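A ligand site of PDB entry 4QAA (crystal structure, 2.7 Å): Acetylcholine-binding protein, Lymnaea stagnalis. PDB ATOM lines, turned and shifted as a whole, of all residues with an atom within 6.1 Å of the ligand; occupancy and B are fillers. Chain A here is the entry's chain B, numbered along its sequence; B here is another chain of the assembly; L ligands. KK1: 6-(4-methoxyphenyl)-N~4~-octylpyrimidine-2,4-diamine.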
ATOM      1  N   TYR A  97     -36.592 -27.183  14.580  1.00  0.00           N
ATOM      2  CA  TYR A  97     -36.038 -27.406  13.225  1.00  0.00           C
ATOM      3  C   TYR A  97     -37.026 -28.057  12.237  1.00  0.00           C
ATOM      4  O   TYR A  97     -37.000 -27.753  11.048  1.00  0.00           O
ATOM      5  CB  TYR A  97     -34.712 -28.171  13.257  1.00  0.00           C
ATOM      6  CG  TYR A  97     -33.606 -27.478  14.083  1.00  0.00           C
ATOM      7  CD1 TYR A  97     -33.702 -26.137  14.416  1.00  0.00           C
ATOM      8  CD2 TYR A  97     -32.489 -28.179  14.520  1.00  0.00           C
ATOM      9  CE1 TYR A  97     -32.708 -25.514  15.146  1.00  0.00           C
ATOM     10  CE2 TYR A  97     -31.495 -27.561  15.259  1.00  0.00           C
ATOM     11  CZ  TYR A  97     -31.601 -26.230  15.566  1.00  0.00           C
ATOM     12  OH  TYR A  97     -30.610 -25.596  16.324  1.00  0.00           O
ATOM     13  N   LYS A 147     -36.446 -31.250  17.237  1.00  0.00           N
ATOM     14  CA  LYS A 147     -35.225 -30.574  17.661  1.00  0.00           C
ATOM     15  C   LYS A 147     -35.480 -29.094  17.957  1.00  0.00           C
ATOM     16  O   LYS A 147     -35.909 -28.332  17.098  1.00  0.00           O
ATOM     17  CB  LYS A 147     -34.118 -30.746  16.632  1.00  0.00           C
ATOM     18  CG  LYS A 147     -33.477 -32.120  16.639  1.00  0.00           C
ATOM     19  CD  LYS A 147     -32.152 -32.134  15.867  1.00  0.00           C
ATOM     20  CE  LYS A 147     -31.661 -33.565  15.663  1.00  0.00           C
ATOM     21  NZ  LYS A 147     -30.491 -33.626  14.763  1.00  0.00           N
ATOM     22  N   GLY A 149     -33.518 -25.814  19.305  1.00  0.00           N
ATOM     23  CA  GLY A 149     -32.213 -25.213  19.522  1.00  0.00           C
ATOM     24  C   GLY A 149     -32.233 -23.706  19.332  1.00  0.00           C
ATOM     25  O   GLY A 149     -33.267 -23.142  18.969  1.00  0.00           O
ATOM     26  N   SER A 150     -31.089 -23.046  19.584  1.00  0.00           N
ATOM     27  CA  SER A 150     -30.954 -21.621  19.260  1.00  0.00           C
ATOM     28  C   SER A 150     -30.878 -21.428  17.770  1.00  0.00           C
ATOM     29  O   SER A 150     -30.095 -22.081  17.099  1.00  0.00           O
ATOM     30  CB  SER A 150     -29.693 -21.015  19.882  1.00  0.00           C
ATOM     31  OG  SER A 150     -29.488 -19.673  19.424  1.00  0.00           O
ATOM     32  N   TRP A 151     -31.681 -20.500  17.263  1.00  0.00           N
ATOM     33  CA  TRP A 151     -31.702 -20.210  15.837  1.00  0.00           C
ATOM     34  C   TRP A 151     -30.472 -19.417  15.349  1.00  0.00           C
ATOM     35  O   TRP A 151     -29.887 -19.778  14.338  1.00  0.00           O
ATOM     36  CB  TRP A 151     -33.004 -19.533  15.450  1.00  0.00           C
ATOM     37  CG  TRP A 151     -33.151 -19.317  13.992  1.00  0.00           C
ATOM     38  CD1 TRP A 151     -33.171 -18.127  13.337  1.00  0.00           C
ATOM     39  CD2 TRP A 151     -33.275 -20.321  12.986  1.00  0.00           C
ATOM     40  NE1 TRP A 151     -33.314 -18.311  11.984  1.00  0.00           N
ATOM     41  CE2 TRP A 151     -33.389 -19.659  11.744  1.00  0.00           C
ATOM     42  CE3 TRP A 151     -33.321 -21.714  13.012  1.00  0.00           C
ATOM     43  CZ2 TRP A 151     -33.535 -20.346  10.548  1.00  0.00           C
ATOM     44  CZ3 TRP A 151     -33.474 -22.394  11.820  1.00  0.00           C
ATOM     45  CH2 TRP A 151     -33.575 -21.705  10.601  1.00  0.00           C
ATOM     46  N   THR A 152     -30.070 -18.351  16.062  1.00  0.00           N
ATOM     47  CA  THR A 152     -28.975 -17.490  15.580  1.00  0.00           C
ATOM     48  C   THR A 152     -27.663 -17.602  16.374  1.00  0.00           C
ATOM     49  O   THR A 152     -26.615 -17.184  15.890  1.00  0.00           O
ATOM     50  CB  THR A 152     -29.388 -15.987  15.471  1.00  0.00           C
ATOM     51  OG1 THR A 152     -29.597 -15.421  16.766  1.00  0.00           O
ATOM     52  CG2 THR A 152     -30.658 -15.822  14.668  1.00  0.00           C
ATOM     53  N   ASN A 189     -27.773 -32.672  21.604  1.00  0.00           N
ATOM     54  CA  ASN A 189     -27.433 -32.909  20.207  1.00  0.00           C
ATOM     55  C   ASN A 189     -26.801 -31.623  19.649  1.00  0.00           C
ATOM     56  O   ASN A 189     -26.970 -30.551  20.222  1.00  0.00           O
ATOM     57  CB  ASN A 189     -28.707 -33.263  19.430  1.00  0.00           C
ATOM     58  CG  ASN A 189     -28.439 -33.803  18.044  1.00  0.00           C
ATOM     59  OD1 ASN A 189     -28.468 -33.064  17.058  1.00  0.00           O
ATOM     60  ND2 ASN A 189     -28.192 -35.105  17.957  1.00  0.00           N
ATOM     61  N   VAL A 191     -26.039 -29.696  15.805  1.00  0.00           N
ATOM     62  CA  VAL A 191     -26.108 -29.653  14.349  1.00  0.00           C
ATOM     63  C   VAL A 191     -24.882 -28.968  13.742  1.00  0.00           C
ATOM     64  O   VAL A 191     -24.275 -28.093  14.365  1.00  0.00           O
ATOM     65  CB  VAL A 191     -27.363 -28.864  13.926  1.00  0.00           C
ATOM     66  CG1 VAL A 191     -27.532 -28.836  12.422  1.00  0.00           C
ATOM     67  CG2 VAL A 191     -28.586 -29.450  14.591  1.00  0.00           C
ATOM     68  N   THR A 192     -24.496 -29.390  12.531  1.00  0.00           N
ATOM     69  CA  THR A 192     -23.439 -28.738  11.771  1.00  0.00           C
ATOM     70  C   THR A 192     -23.655 -28.997  10.285  1.00  0.00           C
ATOM     71  O   THR A 192     -24.294 -28.214   9.590  1.00  0.00           O
ATOM     72  CB  THR A 192     -22.031 -29.243  12.159  1.00  0.00           C
ATOM     73  OG1 THR A 192     -22.145 -30.541  12.756  1.00  0.00           O
ATOM     74  CG2 THR A 192     -21.397 -28.330  13.156  1.00  0.00           C
ATOM     75  N   TYR A 200     -24.515 -25.660  16.292  1.00  0.00           N
ATOM     76  CA  TYR A 200     -25.620 -25.183  17.114  1.00  0.00           C
ATOM     77  C   TYR A 200     -26.112 -26.321  17.960  1.00  0.00           C
ATOM     78  O   TYR A 200     -26.431 -27.391  17.441  1.00  0.00           O
ATOM     79  CB  TYR A 200     -26.764 -24.646  16.252  1.00  0.00           C
ATOM     80  CG  TYR A 200     -26.350 -23.519  15.359  1.00  0.00           C
ATOM     81  CD1 TYR A 200     -25.615 -23.767  14.208  1.00  0.00           C
ATOM     82  CD2 TYR A 200     -26.667 -22.208  15.664  1.00  0.00           C
ATOM     83  CE1 TYR A 200     -25.207 -22.756  13.392  1.00  0.00           C
ATOM     84  CE2 TYR A 200     -26.271 -21.177  14.847  1.00  0.00           C
ATOM     85  CZ  TYR A 200     -25.548 -21.465  13.700  1.00  0.00           C
ATOM     86  OH  TYR A 200     -25.123 -20.471  12.864  1.00  0.00           O
ATOM     87  N   GLU A 201     -26.143 -26.115  19.262  1.00  0.00           N
ATOM     88  CA  GLU A 201     -26.684 -27.106  20.149  1.00  0.00           C
ATOM     89  C   GLU A 201     -28.207 -27.059  20.111  1.00  0.00           C
ATOM     90  O   GLU A 201     -28.805 -26.019  19.794  1.00  0.00           O
ATOM     91  CB  GLU A 201     -26.206 -26.875  21.566  1.00  0.00           C
ATOM     92  CG  GLU A 201     -24.724 -26.837  21.670  1.00  0.00           C
ATOM     93  CD  GLU A 201     -24.268 -26.854  23.100  1.00  0.00           C
ATOM     94  OE1 GLU A 201     -25.120 -27.008  24.006  1.00  0.00           O
ATOM     95  OE2 GLU A 201     -23.054 -26.708  23.323  1.00  0.00           O
ATOM     96  N   ASP A 202     -28.820 -28.185  20.445  1.00  0.00           N
ATOM     97  CA  ASP A 202     -30.260 -28.315  20.451  1.00  0.00           C
ATOM     98  C   ASP A 202     -30.609 -29.442  21.419  1.00  0.00           C
ATOM     99  O   ASP A 202     -29.747 -30.215  21.832  1.00  0.00           O
ATOM    100  CB  ASP A 202     -30.763 -28.642  19.044  1.00  0.00           C
ATOM    101  CG  ASP A 202     -30.607 -30.112  18.679  1.00  0.00           C
ATOM    102  OD1 ASP A 202     -31.524 -30.918  19.014  1.00  0.00           O
ATOM    103  OD2 ASP A 202     -29.575 -30.475  18.060  1.00  0.00           O
ATOM    104  N   TRP B  61     -35.418 -22.468   3.974  1.00  0.00           N
ATOM    105  CA  TRP B  61     -34.588 -21.506   4.653  1.00  0.00           C
ATOM    106  C   TRP B  61     -34.079 -20.533   3.615  1.00  0.00           C
ATOM    107  O   TRP B  61     -33.360 -20.927   2.693  1.00  0.00           O
ATOM    108  CB  TRP B  61     -33.440 -22.196   5.384  1.00  0.00           C
ATOM    109  CG  TRP B  61     -33.962 -23.041   6.507  1.00  0.00           C
ATOM    110  CD1 TRP B  61     -35.269 -23.170   6.909  1.00  0.00           C
ATOM    111  CD2 TRP B  61     -33.201 -23.868   7.399  1.00  0.00           C
ATOM    112  NE1 TRP B  61     -35.362 -24.036   7.972  1.00  0.00           N
ATOM    113  CE2 TRP B  61     -34.110 -24.483   8.294  1.00  0.00           C
ATOM    114  CE3 TRP B  61     -31.838 -24.169   7.509  1.00  0.00           C
ATOM    115  CZ2 TRP B  61     -33.704 -25.365   9.295  1.00  0.00           C
ATOM    116  CZ3 TRP B  61     -31.432 -25.043   8.492  1.00  0.00           C
ATOM    117  CH2 TRP B  61     -32.360 -25.627   9.380  1.00  0.00           C
ATOM    118  N   LEU B 110     -34.219 -12.566  13.578  1.00  0.00           N
ATOM    119  CA  LEU B 110     -32.948 -11.998  13.992  1.00  0.00           C
ATOM    120  C   LEU B 110     -31.920 -12.114  12.893  1.00  0.00           C
ATOM    121  O   LEU B 110     -31.867 -13.107  12.197  1.00  0.00           O
ATOM    122  CB  LEU B 110     -32.430 -12.671  15.280  1.00  0.00           C
ATOM    123  CG  LEU B 110     -33.222 -12.471  16.566  1.00  0.00           C
ATOM    124  CD1 LEU B 110     -32.697 -13.393  17.643  1.00  0.00           C
ATOM    125  CD2 LEU B 110     -33.032 -11.047  17.006  1.00  0.00           C
ATOM    126  N   ALA B 111     -31.118 -11.089  12.703  1.00  0.00           N
ATOM    127  CA  ALA B 111     -30.076 -11.177  11.706  1.00  0.00           C
ATOM    128  C   ALA B 111     -28.767 -11.317  12.442  1.00  0.00           C
ATOM    129  O   ALA B 111     -28.704 -11.159  13.662  1.00  0.00           O
ATOM    130  CB  ALA B 111     -30.076  -9.940  10.828  1.00  0.00           C
ATOM    131  N   ARG B 112     -27.713 -11.653  11.724  1.00  0.00           N
ATOM    132  CA  ARG B 112     -26.398 -11.629  12.317  1.00  0.00           C
ATOM    133  C   ARG B 112     -25.630 -10.523  11.622  1.00  0.00           C
ATOM    134  O   ARG B 112     -25.724 -10.360  10.404  1.00  0.00           O
ATOM    135  CB  ARG B 112     -25.704 -12.986  12.186  1.00  0.00           C
ATOM    136  CG  ARG B 112     -26.431 -14.119  12.889  1.00  0.00           C
ATOM    137  CD  ARG B 112     -26.157 -14.104  14.398  1.00  0.00           C
ATOM    138  NE  ARG B 112     -24.775 -14.461  14.703  1.00  0.00           N
ATOM    139  CZ  ARG B 112     -24.280 -14.578  15.928  1.00  0.00           C
ATOM    140  NH1 ARG B 112     -25.070 -14.357  16.990  1.00  0.00           N
ATOM    141  NH2 ARG B 112     -23.006 -14.909  16.116  1.00  0.00           N
ATOM    142  N   LEU B 120     -26.176 -11.161   7.652  1.00  0.00           N
ATOM    143  CA  LEU B 120     -26.699 -12.471   7.325  1.00  0.00           C
ATOM    144  C   LEU B 120     -28.070 -12.600   7.952  1.00  0.00           C
ATOM    145  O   LEU B 120     -28.220 -12.465   9.147  1.00  0.00           O
ATOM    146  CB  LEU B 120     -25.779 -13.522   7.934  1.00  0.00           C
ATOM    147  CG  LEU B 120     -24.301 -13.173   7.755  1.00  0.00           C
ATOM    148  CD1 LEU B 120     -23.510 -13.733   8.909  1.00  0.00           C
ATOM    149  CD2 LEU B 120     -23.805 -13.743   6.468  1.00  0.00           C
ATOM    150  N   TYR B 121     -29.078 -12.850   7.125  1.00  0.00           N
ATOM    151  CA  TYR B 121     -30.415 -13.065   7.620  1.00  0.00           C
ATOM    152  C   TYR B 121     -31.033 -14.284   6.941  1.00  0.00           C
ATOM    153  O   TYR B 121     -31.139 -14.317   5.705  1.00  0.00           O
ATOM    154  CB  TYR B 121     -31.265 -11.838   7.349  1.00  0.00           C
ATOM    155  CG  TYR B 121     -32.715 -11.998   7.719  1.00  0.00           C
ATOM    156  CD1 TYR B 121     -33.087 -12.348   9.011  1.00  0.00           C
ATOM    157  CD2 TYR B 121     -33.722 -11.796   6.778  1.00  0.00           C
ATOM    158  CE1 TYR B 121     -34.408 -12.489   9.362  1.00  0.00           C
ATOM    159  CE2 TYR B 121     -35.060 -11.936   7.098  1.00  0.00           C
ATOM    160  CZ  TYR B 121     -35.396 -12.287   8.398  1.00  0.00           C
ATOM    161  OH  TYR B 121     -36.723 -12.422   8.754  1.00  0.00           O
ATOM    162  N   MET B 122     -31.434 -15.277   7.732  1.00  0.00           N
ATOM    163  CA  MET B 122     -31.964 -16.540   7.195  1.00  0.00           C
ATOM    164  C   MET B 122     -33.204 -17.015   7.915  1.00  0.00           C
ATOM    165  O   MET B 122     -33.116 -17.877   8.772  1.00  0.00           O
ATOM    166  CB  MET B 122     -30.902 -17.637   7.286  1.00  0.00           C
ATOM    167  CG  MET B 122     -31.246 -18.875   6.432  1.00  0.00           C
ATOM    168  SD  MET B 122     -30.110 -20.295   6.508  1.00  0.00           S
ATOM    169  CE  MET B 122     -30.415 -20.963   8.142  1.00  0.00           C
ATOM    170  N   GLU B 171     -28.898 -32.102   2.389  1.00  0.00           N
ATOM    171  CA  GLU B 171     -28.580 -31.763   3.721  1.00  0.00           C
ATOM    172  C   GLU B 171     -29.758 -31.388   4.517  1.00  0.00           C
ATOM    173  O   GLU B 171     -29.840 -31.790   5.616  1.00  0.00           O
ATOM    174  CB  GLU B 171     -27.512 -30.732   3.756  1.00  0.00           C
ATOM    175  CG  GLU B 171     -26.339 -31.162   4.568  1.00  0.00           C
ATOM    176  CD  GLU B 171     -25.145 -30.316   4.297  1.00  0.00           C
ATOM    177  OE1 GLU B 171     -24.895 -29.999   3.117  1.00  0.00           O
ATOM    178  OE2 GLU B 171     -24.441 -29.965   5.251  1.00  0.00           O
ATOM    179  N   TYR B 172     -30.661 -30.610   3.975  1.00  0.00           N
ATOM    180  CA  TYR B 172     -31.706 -30.030   4.777  1.00  0.00           C
ATOM    181  C   TYR B 172     -33.090 -30.562   4.541  1.00  0.00           C
ATOM    182  O   TYR B 172     -33.960 -30.367   5.339  1.00  0.00           O
ATOM    183  CB  TYR B 172     -31.726 -28.509   4.639  1.00  0.00           C
ATOM    184  CG  TYR B 172     -30.409 -27.835   4.602  1.00  0.00           C
ATOM    185  CD1 TYR B 172     -29.936 -27.312   3.458  1.00  0.00           C
ATOM    186  CD2 TYR B 172     -29.634 -27.775   5.690  1.00  0.00           C
ATOM    187  CE1 TYR B 172     -28.719 -26.742   3.407  1.00  0.00           C
ATOM    188  CE2 TYR B 172     -28.412 -27.229   5.639  1.00  0.00           C
ATOM    189  CZ  TYR B 172     -27.968 -26.702   4.498  1.00  0.00           C
ATOM    190  OH  TYR B 172     -26.750 -26.136   4.457  1.00  0.00           O
HETATM  191  C01 KK1 L   1     -29.092 -32.863  11.562  1.00  0.00           C
HETATM  192  C02 KK1 L   1     -30.030 -31.873  12.281  1.00  0.00           C
HETATM  193  C03 KK1 L   1     -31.387 -31.672  11.566  1.00  0.00           C
HETATM  194  C04 KK1 L   1     -31.819 -30.162  11.549  1.00  0.00           C
HETATM  195  C05 KK1 L   1     -31.370 -29.401  10.232  1.00  0.00           C
HETATM  196  C06 KK1 L   1     -30.449 -28.126  10.504  1.00  0.00           C
HETATM  197  C07 KK1 L   1     -29.361 -27.788   9.378  1.00  0.00           C
HETATM  198  C08 KK1 L   1     -28.600 -26.361   9.507  1.00  0.00           C
HETATM  199  N09 KK1 L   1     -28.289 -25.922  10.931  1.00  0.00           N
HETATM  200  C10 KK1 L   1     -28.669 -24.653  11.597  1.00  0.00           C
HETATM  201  C11 KK1 L   1     -28.396 -23.323  10.975  1.00  0.00           C
HETATM  202  C12 KK1 L   1     -28.784 -22.158  11.746  1.00  0.00           C
HETATM  203  N13 KK1 L   1     -29.346 -22.314  12.983  1.00  0.00           N
HETATM  204  C14 KK1 L   1     -29.562 -23.553  13.492  1.00  0.00           C
HETATM  205  N15 KK1 L   1     -30.147 -23.656  14.778  1.00  0.00           N
HETATM  206  N16 KK1 L   1     -29.248 -24.738  12.858  1.00  0.00           N
HETATM  207  C17 KK1 L   1     -28.616 -20.612  11.323  1.00  0.00           C
HETATM  208  C18 KK1 L   1     -27.372 -20.025  11.013  1.00  0.00           C
HETATM  209  C19 KK1 L   1     -27.181 -18.602  10.673  1.00  0.00           C
HETATM  210  C20 KK1 L   1     -28.294 -17.734  10.650  1.00  0.00           C
HETATM  211  O21 KK1 L   1     -28.164 -16.413  10.330  1.00  0.00           O
HETATM  212  C22 KK1 L   1     -29.213 -15.553  10.879  1.00  0.00           C
HETATM  213  C23 KK1 L   1     -29.539 -18.289  10.976  1.00  0.00           C
HETATM  214  C24 KK1 L   1     -29.677 -19.678  11.307  1.00  0.00           C
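The side-chain hydroxyl (OH) of Tyr 97 is in hydrogen-bond range of a nitrogen (N15) of the ligand (2.5 Å). A nitrogen (N15) of the ligand is in hydrogen-bond range of the backbone carbonyl oxygen (O) of Ser 150.
N13 of the ligand lies close to O of Trp 151 (2.9 Å). Lys 147 touches the ligand. Val 191 touches the ligand. Tyr 200 touches the ligand (OH to C18, 2.9 Å). CZ3 of Trp 61 of chain B touches C08 of the ligand, 3.3 Å away. Leu 110 of chain B touches the ligand (O to C22, 3.8 Å). Arg 112 of chain B touches the ligand (CG to C22, 3.7 Å). Leu 120 of chain B touches the ligand. Met 122 of chain B touches the ligand. CD2 of Tyr 172 of chain B touches C07 of the ligand (3.7 Å). Hydrophobic or aromatic side chains that line the ligand: Tyr 97, Trp 151, Val 191, Tyr 200, Trp 61 of chain B, Met 122 of chain B and Tyr 172 of chain B.
O of Lys 147 sits at hydrogen-bond distance from N of Tyr 97 (2.9 Å). O of Tyr 200 is in hydrogen-bond range of N of Val 191. The side-chain amino group (NZ) of Lys 147 sits at hydrogen-bond distance from the side-chain amide oxygen (OD1) of Asn 189. NE1 of Trp 151 lies close to O of Met 122 of chain B. NH1 of Arg 112 of chain B lies within hydrogen-bond range of O of Thr 152 (3.4 Å). O of Leu 120 of chain B lies within hydrogen-bond range of N of Arg 112 of chain B, 2.7 Å away.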
